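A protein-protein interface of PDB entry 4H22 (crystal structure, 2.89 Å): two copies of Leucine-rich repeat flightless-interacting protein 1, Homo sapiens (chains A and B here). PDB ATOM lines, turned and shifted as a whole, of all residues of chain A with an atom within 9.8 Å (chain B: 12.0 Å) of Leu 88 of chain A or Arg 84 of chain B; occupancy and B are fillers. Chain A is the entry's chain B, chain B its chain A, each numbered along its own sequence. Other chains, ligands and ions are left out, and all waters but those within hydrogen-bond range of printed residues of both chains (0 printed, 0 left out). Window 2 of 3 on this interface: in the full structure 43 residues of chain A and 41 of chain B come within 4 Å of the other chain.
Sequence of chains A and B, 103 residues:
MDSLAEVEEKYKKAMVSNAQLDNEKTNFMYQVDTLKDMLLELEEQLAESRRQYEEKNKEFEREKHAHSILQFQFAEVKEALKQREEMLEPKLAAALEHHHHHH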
ATOM      1  N   VAL A  77       6.547 -12.134  28.319  1.00  0.00           N
ATOM      2  CA  VAL A  77       7.353 -11.236  27.487  1.00  0.00           C
ATOM      3  C   VAL A  77       8.253 -10.313  28.314  1.00  0.00           C
ATOM      4  O   VAL A  77       9.370 -10.015  27.908  1.00  0.00           O
ATOM      5  CB  VAL A  77       6.466 -10.445  26.498  1.00  0.00           C
ATOM      6  CG1 VAL A  77       7.101  -9.126  26.086  1.00  0.00           C
ATOM      7  CG2 VAL A  77       6.162 -11.296  25.275  1.00  0.00           C
ATOM      8  N   ALA A  80      11.432 -12.413  28.976  1.00  0.00           N
ATOM      9  CA  ALA A  80      12.291 -12.473  27.795  1.00  0.00           C
ATOM     10  C   ALA A  80      13.040 -11.162  27.600  1.00  0.00           C
ATOM     11  O   ALA A  80      14.251 -11.161  27.417  1.00  0.00           O
ATOM     12  CB  ALA A  80      11.477 -12.813  26.557  1.00  0.00           C
ATOM     13  N   LEU A  81      12.311 -10.050  27.675  1.00  0.00           N
ATOM     14  CA  LEU A  81      12.888  -8.711  27.593  1.00  0.00           C
ATOM     15  C   LEU A  81      14.031  -8.547  28.588  1.00  0.00           C
ATOM     16  O   LEU A  81      15.107  -8.063  28.231  1.00  0.00           O
ATOM     17  CB  LEU A  81      11.798  -7.656  27.840  1.00  0.00           C
ATOM     18  CG  LEU A  81      11.950  -6.169  27.477  1.00  0.00           C
ATOM     19  CD1 LEU A  81      12.648  -5.369  28.572  1.00  0.00           C
ATOM     20  CD2 LEU A  81      12.611  -5.955  26.118  1.00  0.00           C
ATOM     21  N   LYS A  82      13.797  -8.977  29.826  1.00  0.00           N
ATOM     22  CA  LYS A  82      14.798  -8.888  30.881  1.00  0.00           C
ATOM     23  C   LYS A  82      16.023  -9.742  30.574  1.00  0.00           C
ATOM     24  O   LYS A  82      17.124  -9.453  31.057  1.00  0.00           O
ATOM     25  CB  LYS A  82      14.204  -9.286  32.231  1.00  0.00           C
ATOM     26  CG  LYS A  82      14.811  -8.531  33.405  1.00  0.00           C
ATOM     27  CD  LYS A  82      14.840  -9.380  34.667  1.00  0.00           C
ATOM     28  CE  LYS A  82      16.148 -10.161  34.781  1.00  0.00           C
ATOM     29  NZ  LYS A  82      16.150 -11.048  36.057  1.00  0.00           N
ATOM     30  N   GLN A  83      15.826 -10.785  29.765  1.00  0.00           N
ATOM     31  CA  GLN A  83      16.911 -11.704  29.429  1.00  0.00           C
ATOM     32  C   GLN A  83      17.737 -11.251  28.229  1.00  0.00           C
ATOM     33  O   GLN A  83      18.865 -11.714  28.041  1.00  0.00           O
ATOM     34  CB  GLN A  83      16.378 -13.119  29.188  1.00  0.00           C
ATOM     35  CG  GLN A  83      17.301 -14.198  29.727  1.00  0.00           C
ATOM     36  CD  GLN A  83      17.251 -14.300  31.243  1.00  0.00           C
ATOM     37  OE1 GLN A  83      16.187 -14.147  31.846  1.00  0.00           O
ATOM     38  NE2 GLN A  83      18.403 -14.560  31.871  1.00  0.00           N
ATOM     39  N   ARG A  84      17.175 -10.365  27.409  1.00  0.00           N
ATOM     40  CA  ARG A  84      17.925  -9.809  26.286  1.00  0.00           C
ATOM     41  C   ARG A  84      18.801  -8.667  26.784  1.00  0.00           C
ATOM     42  O   ARG A  84      19.892  -8.449  26.265  1.00  0.00           O
ATOM     43  CB  ARG A  84      17.016  -9.333  25.140  1.00  0.00           C
ATOM     44  CG  ARG A  84      15.800 -10.206  24.812  1.00  0.00           C
ATOM     45  CD  ARG A  84      16.065 -11.705  24.891  1.00  0.00           C
ATOM     46  NE  ARG A  84      16.192 -12.335  23.543  1.00  0.00           N
ATOM     47  CZ  ARG A  84      16.585 -13.601  23.327  1.00  0.00           C
ATOM     48  NH1 ARG A  84      16.912 -14.373  24.368  1.00  0.00           N
ATOM     49  NH2 ARG A  84      16.662 -14.099  22.068  1.00  0.00           N
ATOM     50  N   GLU A  85      18.318  -7.954  27.801  1.00  0.00           N
ATOM     51  CA  GLU A  85      19.101  -6.922  28.479  1.00  0.00           C
ATOM     52  C   GLU A  85      20.190  -7.546  29.348  1.00  0.00           C
ATOM     53  O   GLU A  85      21.259  -6.941  29.548  1.00  0.00           O
ATOM     54  CB  GLU A  85      18.201  -6.050  29.351  1.00  0.00           C
ATOM     55  CG  GLU A  85      17.134  -5.282  28.588  1.00  0.00           C
ATOM     56  CD  GLU A  85      16.109  -4.635  29.505  1.00  0.00           C
ATOM     57  OE1 GLU A  85      15.893  -5.142  30.642  1.00  0.00           O
ATOM     58  OE2 GLU A  85      15.510  -3.614  29.085  1.00  0.00           O
ATOM     59  N   GLU A  86      19.918  -8.745  29.862  1.00  0.00           N
ATOM     60  CA  GLU A  86      20.877  -9.510  30.661  1.00  0.00           C
ATOM     61  C   GLU A  86      22.016 -10.039  29.784  1.00  0.00           C
ATOM     62  O   GLU A  86      23.191  -9.869  30.117  1.00  0.00           O
ATOM     63  CB  GLU A  86      20.165 -10.679  31.361  1.00  0.00           C
ATOM     64  CG  GLU A  86      21.010 -11.449  32.369  1.00  0.00           C
ATOM     65  CD  GLU A  86      20.790 -10.990  33.798  1.00  0.00           C
ATOM     66  OE1 GLU A  86      21.794 -10.751  34.504  1.00  0.00           O
ATOM     67  OE2 GLU A  86      19.614 -10.871  34.220  1.00  0.00           O
ATOM     68  N   MET A  87      21.650 -10.659  28.662  1.00  0.00           N
ATOM     69  CA  MET A  87      22.596 -11.327  27.759  1.00  0.00           C
ATOM     70  C   MET A  87      23.701 -10.407  27.227  1.00  0.00           C
ATOM     71  O   MET A  87      24.828 -10.853  26.999  1.00  0.00           O
ATOM     72  CB  MET A  87      21.833 -11.998  26.600  1.00  0.00           C
ATOM     73  CG  MET A  87      22.714 -12.567  25.472  1.00  0.00           C
ATOM     74  SD  MET A  87      21.744 -13.370  24.129  1.00  0.00           S
ATOM     75  CE  MET A  87      23.102 -14.004  23.118  1.00  0.00           C
ATOM     76  N   LEU A  88      23.379  -9.127  27.051  1.00  0.00           N
ATOM     77  CA  LEU A  88      24.317  -8.169  26.465  1.00  0.00           C
ATOM     78  C   LEU A  88      25.265  -7.541  27.497  1.00  0.00           C
ATOM     79  O   LEU A  88      26.412  -7.209  27.171  1.00  0.00           O
ATOM     80  CB  LEU A  88      23.560  -7.099  25.659  1.00  0.00           C
ATOM     81  CG  LEU A  88      22.493  -7.615  24.676  1.00  0.00           C
ATOM     82  CD1 LEU A  88      21.653  -6.471  24.085  1.00  0.00           C
ATOM     83  CD2 LEU A  88      23.104  -8.482  23.562  1.00  0.00           C
ATOM     84  N   GLU A  89      24.787  -7.389  28.733  1.00  0.00           N
ATOM     85  CA  GLU A  89      25.621  -6.898  29.833  1.00  0.00           C
ATOM     86  C   GLU A  89      26.343  -8.062  30.517  1.00  0.00           C
ATOM     87  O   GLU A  89      27.587  -8.104  30.548  1.00  0.00           O
ATOM     88  CB  GLU A  89      24.767  -6.124  30.853  1.00  0.00           C
ATOM     89  CG  GLU A  89      24.539  -4.653  30.500  1.00  0.00           C
ATOM     90  CD  GLU A  89      23.235  -4.107  31.079  1.00  0.00           C
ATOM     91  OE1 GLU A  89      22.384  -4.895  31.641  1.00  0.00           O
ATOM     92  OE2 GLU A  89      23.033  -2.861  30.917  1.00  0.00           O
ATOM     93  N   ALA B  75       1.834  -3.453  24.843  1.00  0.00           N
ATOM     94  CA  ALA B  75       2.171  -2.926  23.526  1.00  0.00           C
ATOM     95  C   ALA B  75       3.577  -2.336  23.492  1.00  0.00           C
ATOM     96  O   ALA B  75       4.289  -2.489  22.499  1.00  0.00           O
ATOM     97  CB  ALA B  75       1.147  -1.892  23.087  1.00  0.00           C
ATOM     98  N   GLU B  76       3.968  -1.674  24.581  1.00  0.00           N
ATOM     99  CA  GLU B  76       5.307  -1.104  24.705  1.00  0.00           C
ATOM    100  C   GLU B  76       6.372  -2.174  24.891  1.00  0.00           C
ATOM    101  O   GLU B  76       7.414  -2.143  24.242  1.00  0.00           O
ATOM    102  CB  GLU B  76       5.369  -0.108  25.859  1.00  0.00           C
ATOM    103  CG  GLU B  76       4.958   1.303  25.477  1.00  0.00           C
ATOM    104  CD  GLU B  76       5.459   2.343  26.461  1.00  0.00           C
ATOM    105  OE1 GLU B  76       6.006   1.954  27.520  1.00  0.00           O
ATOM    106  OE2 GLU B  76       5.311   3.551  26.174  1.00  0.00           O
ATOM    107  N   VAL B  77       6.098  -3.127  25.768  1.00  0.00           N
ATOM    108  CA  VAL B  77       7.063  -4.162  26.100  1.00  0.00           C
ATOM    109  C   VAL B  77       7.187  -5.215  24.993  1.00  0.00           C
ATOM    110  O   VAL B  77       8.212  -5.882  24.888  1.00  0.00           O
ATOM    111  CB  VAL B  77       6.750  -4.785  27.483  1.00  0.00           C
ATOM    112  CG1 VAL B  77       7.707  -5.919  27.825  1.00  0.00           C
ATOM    113  CG2 VAL B  77       6.822  -3.716  28.567  1.00  0.00           C
ATOM    114  N   LYS B  78       6.168  -5.347  24.148  1.00  0.00           N
ATOM    115  CA  LYS B  78       6.261  -6.264  23.006  1.00  0.00           C
ATOM    116  C   LYS B  78       7.013  -5.643  21.827  1.00  0.00           C
ATOM    117  O   LYS B  78       7.605  -6.362  21.020  1.00  0.00           O
ATOM    118  CB  LYS B  78       4.884  -6.789  22.573  1.00  0.00           C
ATOM    119  CG  LYS B  78       4.048  -5.829  21.735  1.00  0.00           C
ATOM    120  CD  LYS B  78       2.911  -6.547  21.021  1.00  0.00           C
ATOM    121  CE  LYS B  78       3.398  -7.289  19.784  1.00  0.00           C
ATOM    122  NZ  LYS B  78       2.311  -8.062  19.121  1.00  0.00           N
ATOM    123  N   GLU B  79       6.988  -4.315  21.734  1.00  0.00           N
ATOM    124  CA  GLU B  79       7.725  -3.606  20.691  1.00  0.00           C
ATOM    125  C   GLU B  79       9.163  -3.328  21.101  1.00  0.00           C
ATOM    126  O   GLU B  79      10.049  -3.239  20.250  1.00  0.00           O
ATOM    127  CB  GLU B  79       7.016  -2.315  20.285  1.00  0.00           C
ATOM    128  CG  GLU B  79       5.981  -2.520  19.189  1.00  0.00           C
ATOM    129  CD  GLU B  79       5.716  -1.257  18.392  1.00  0.00           C
ATOM    130  OE1 GLU B  79       5.057  -0.334  18.931  1.00  0.00           O
ATOM    131  OE2 GLU B  79       6.158  -1.190  17.220  1.00  0.00           O
ATOM    132  N   ALA B  80       9.388  -3.200  22.405  1.00  0.00           N
ATOM    133  CA  ALA B  80      10.742  -3.102  22.943  1.00  0.00           C
ATOM    134  C   ALA B  80      11.469  -4.446  22.873  1.00  0.00           C
ATOM    135  O   ALA B  80      12.700  -4.488  22.917  1.00  0.00           O
ATOM    136  CB  ALA B  80      10.715  -2.580  24.371  1.00  0.00           C
ATOM    137  N   LEU B  81      10.705  -5.534  22.761  1.00  0.00           N
ATOM    138  CA  LEU B  81      11.273  -6.881  22.628  1.00  0.00           C
ATOM    139  C   LEU B  81      11.558  -7.248  21.178  1.00  0.00           C
ATOM    140  O   LEU B  81      12.483  -8.013  20.906  1.00  0.00           O
ATOM    141  CB  LEU B  81      10.359  -7.940  23.263  1.00  0.00           C
ATOM    142  CG  LEU B  81      10.836  -9.404  23.285  1.00  0.00           C
ATOM    143  CD1 LEU B  81      11.950  -9.618  24.304  1.00  0.00           C
ATOM    144  CD2 LEU B  81       9.684 -10.367  23.545  1.00  0.00           C
ATOM    145  N   LYS B  82      10.767  -6.713  20.250  1.00  0.00           N
ATOM    146  CA  LYS B  82      10.979  -7.000  18.835  1.00  0.00           C
ATOM    147  C   LYS B  82      12.327  -6.460  18.347  1.00  0.00           C
ATOM    148  O   LYS B  82      12.977  -7.077  17.499  1.00  0.00           O
ATOM    149  CB  LYS B  82       9.824  -6.484  17.968  1.00  0.00           C
ATOM    150  CG  LYS B  82       9.657  -7.285  16.684  1.00  0.00           C
ATOM    151  CD  LYS B  82       8.385  -6.938  15.915  1.00  0.00           C
ATOM    152  CE  LYS B  82       8.197  -7.890  14.738  1.00  0.00           C
ATOM    153  NZ  LYS B  82       6.922  -7.657  13.984  1.00  0.00           N
ATOM    154  N   GLN B  83      12.754  -5.331  18.916  1.00  0.00           N
ATOM    155  CA  GLN B  83      14.025  -4.690  18.554  1.00  0.00           C
ATOM    156  C   GLN B  83      15.263  -5.392  19.117  1.00  0.00           C
ATOM    157  O   GLN B  83      16.393  -4.984  18.833  1.00  0.00           O
ATOM    158  CB  GLN B  83      14.027  -3.228  18.996  1.00  0.00           C
ATOM    159  CG  GLN B  83      13.031  -2.358  18.255  1.00  0.00           C
ATOM    160  CD  GLN B  83      13.220  -0.888  18.559  1.00  0.00           C
ATOM    161  OE1 GLN B  83      14.043  -0.510  19.402  1.00  0.00           O
ATOM    162  NE2 GLN B  83      12.460  -0.044  17.868  1.00  0.00           N
ATOM    163  N   ARG B  84      15.041  -6.433  19.918  1.00  0.00           N
ATOM    164  CA  ARG B  84      16.125  -7.248  20.473  1.00  0.00           C
ATOM    165  C   ARG B  84      15.964  -8.738  20.150  1.00  0.00           C
ATOM    166  O   ARG B  84      16.643  -9.585  20.732  1.00  0.00           O
ATOM    167  CB  ARG B  84      16.254  -7.029  21.985  1.00  0.00           C
ATOM    168  CG  ARG B  84      16.805  -5.665  22.370  1.00  0.00           C
ATOM    169  CD  ARG B  84      16.783  -5.470  23.877  1.00  0.00           C
ATOM    170  NE  ARG B  84      16.887  -4.058  24.241  1.00  0.00           N
ATOM    171  CZ  ARG B  84      18.023  -3.436  24.545  1.00  0.00           C
ATOM    172  NH1 ARG B  84      19.175  -4.094  24.537  1.00  0.00           N
ATOM    173  NH2 ARG B  84      18.005  -2.150  24.862  1.00  0.00           N
ATOM    174  N   GLU B  85      15.054  -9.044  19.227  1.00  0.00           N
ATOM    175  CA  GLU B  85      14.938 -10.382  18.646  1.00  0.00           C
ATOM    176  C   GLU B  85      15.132 -10.325  17.135  1.00  0.00           C
ATOM    177  O   GLU B  85      15.476 -11.328  16.508  1.00  0.00           O
ATOM    178  CB  GLU B  85      13.600 -11.027  19.007  1.00  0.00           C
ATOM    179  CG  GLU B  85      13.622 -11.744  20.349  1.00  0.00           C
ATOM    180  CD  GLU B  85      12.285 -12.360  20.724  1.00  0.00           C
ATOM    181  OE1 GLU B  85      11.252 -11.653  20.652  1.00  0.00           O
ATOM    182  OE2 GLU B  85      12.269 -13.554  21.108  1.00  0.00           O
ATOM    183  N   GLU B  86      14.907  -9.142  16.563  1.00  0.00           N
ATOM    184  CA  GLU B  86      15.328  -8.838  15.197  1.00  0.00           C
ATOM    185  C   GLU B  86      16.824  -8.528  15.164  1.00  0.00           C
ATOM    186  O   GLU B  86      17.415  -8.392  14.092  1.00  0.00           O
ATOM    187  CB  GLU B  86      14.534  -7.658  14.629  1.00  0.00           C
ATOM    188  CG  GLU B  86      13.182  -8.035  14.043  1.00  0.00           C
ATOM    189  CD  GLU B  86      12.455  -6.855  13.424  1.00  0.00           C
ATOM    190  OE1 GLU B  86      13.117  -5.874  13.017  1.00  0.00           O
ATOM    191  OE2 GLU B  86      11.211  -6.911  13.340  1.00  0.00           O
ATOM    192  N   MET B  87      17.422  -8.411  16.349  1.00  0.00           N
ATOM    193  CA  MET B  87      18.861  -8.210  16.495  1.00  0.00           C
ATOM    194  C   MET B  87      19.599  -9.553  16.605  1.00  0.00           C
ATOM    195  O   MET B  87      20.831  -9.593  16.575  1.00  0.00           O
ATOM    196  CB  MET B  87      19.150  -7.334  17.721  1.00  0.00           C
ATOM    197  CG  MET B  87      20.413  -6.488  17.619  1.00  0.00           C
ATOM    198  SD  MET B  87      20.175  -4.920  16.752  1.00  0.00           S
ATOM    199  CE  MET B  87      19.439  -3.907  18.041  1.00  0.00           C
ATOM    200  N   LEU B  88      18.839 -10.644  16.718  1.00  0.00           N
ATOM    201  CA  LEU B  88      19.405 -11.987  16.867  1.00  0.00           C
ATOM    202  C   LEU B  88      19.077 -12.928  15.708  1.00  0.00           C
ATOM    203  O   LEU B  88      18.120 -12.694  14.954  1.00  0.00           O
ATOM    204  CB  LEU B  88      18.963 -12.615  18.191  1.00  0.00           C
ATOM    205  CG  LEU B  88      19.735 -12.169  19.441  1.00  0.00           C
ATOM    206  CD1 LEU B  88      18.795 -12.103  20.644  1.00  0.00           C
ATOM    207  CD2 LEU B  88      20.910 -13.103  19.718  1.00  0.00           C
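Val 77 of chain B touches its own counterpart, Val 77 of chain A. Leu 81 of chain A touches its own counterpart, Leu 81 of chain B. Arg 84 of chain A touches Leu 81 of chain B, but with the chains exchanged Leu 81 of chain A does not touch Arg 84 of chain B (4.8 Å). Arg 84 of chain A touches Leu 88 of chain B, and with the chains exchanged Leu 88 of chain A touches Arg 84 of chain B. Positions printed for both chains: 77, 80, 81, 82, 83, 84, 85, 86, 87 and 88.
Hydrophobic or aromatic side chains of chain A within 4 Å of the printed part of chain B: Val 77, Ala 80, Leu 81 and Leu 88. Hydrophobic or aromatic side chains of chain B that line the printed part of chain A: Val 77, Leu 81 and Leu 88.
Of chain A, only Arg 84 (3.96 Å) and Leu 88 (3.5 Å) come within 4 Å of Arg 84 of chain B. Leu 81 of chain A touches two residues of chain B. Arg 84 of chain A touches just these residues of chain B: Leu 81, Arg 84 and Leu 88. Glu 85 of chain A touches none of the printed residues of chain B. Met 87 of chain A touches none of the printed residues of chain B. No residue of chain B comes within 4 Å of Glu 89 of chain A. Printed residues of chain B within 4 Å of Ala 80 of chain A: Leu 81 (3.8 Å). Of the printed residues of chain B, Val 77 of chain A touches Val 77 and Leu 81. Gln 83 of chain B touches none of the printed residues of chain A. Ala 75 of chain B touches none of the printed residues of chain A. The nearest residue of chain A that does not touch Arg 84 of chain B is Glu 85 of chain A (4.5 Å). The nearest printed residue of chain A that does not touch Ala 80 of chain B is Arg 84 of chain A (6.8 Å).
Among the printed residues, merely in contact across the chains: Arg 84 of chain A with Leu 88 of chain B, Leu 81 of chain A with Leu 81 of chain B, Leu 88 of chain A with Arg 84 of chain B, Leu 81 of chain A with Ala 80 of chain B, Val 77 of chain A with Val 77 of chain B, Ala 80 of chain A with Leu 81 of chain B, Val 77 of chain A with Leu 81 of chain B, Arg 84 of chain A with Leu 81 of chain B and Arg 84 of chain A with Arg 84 of chain B.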
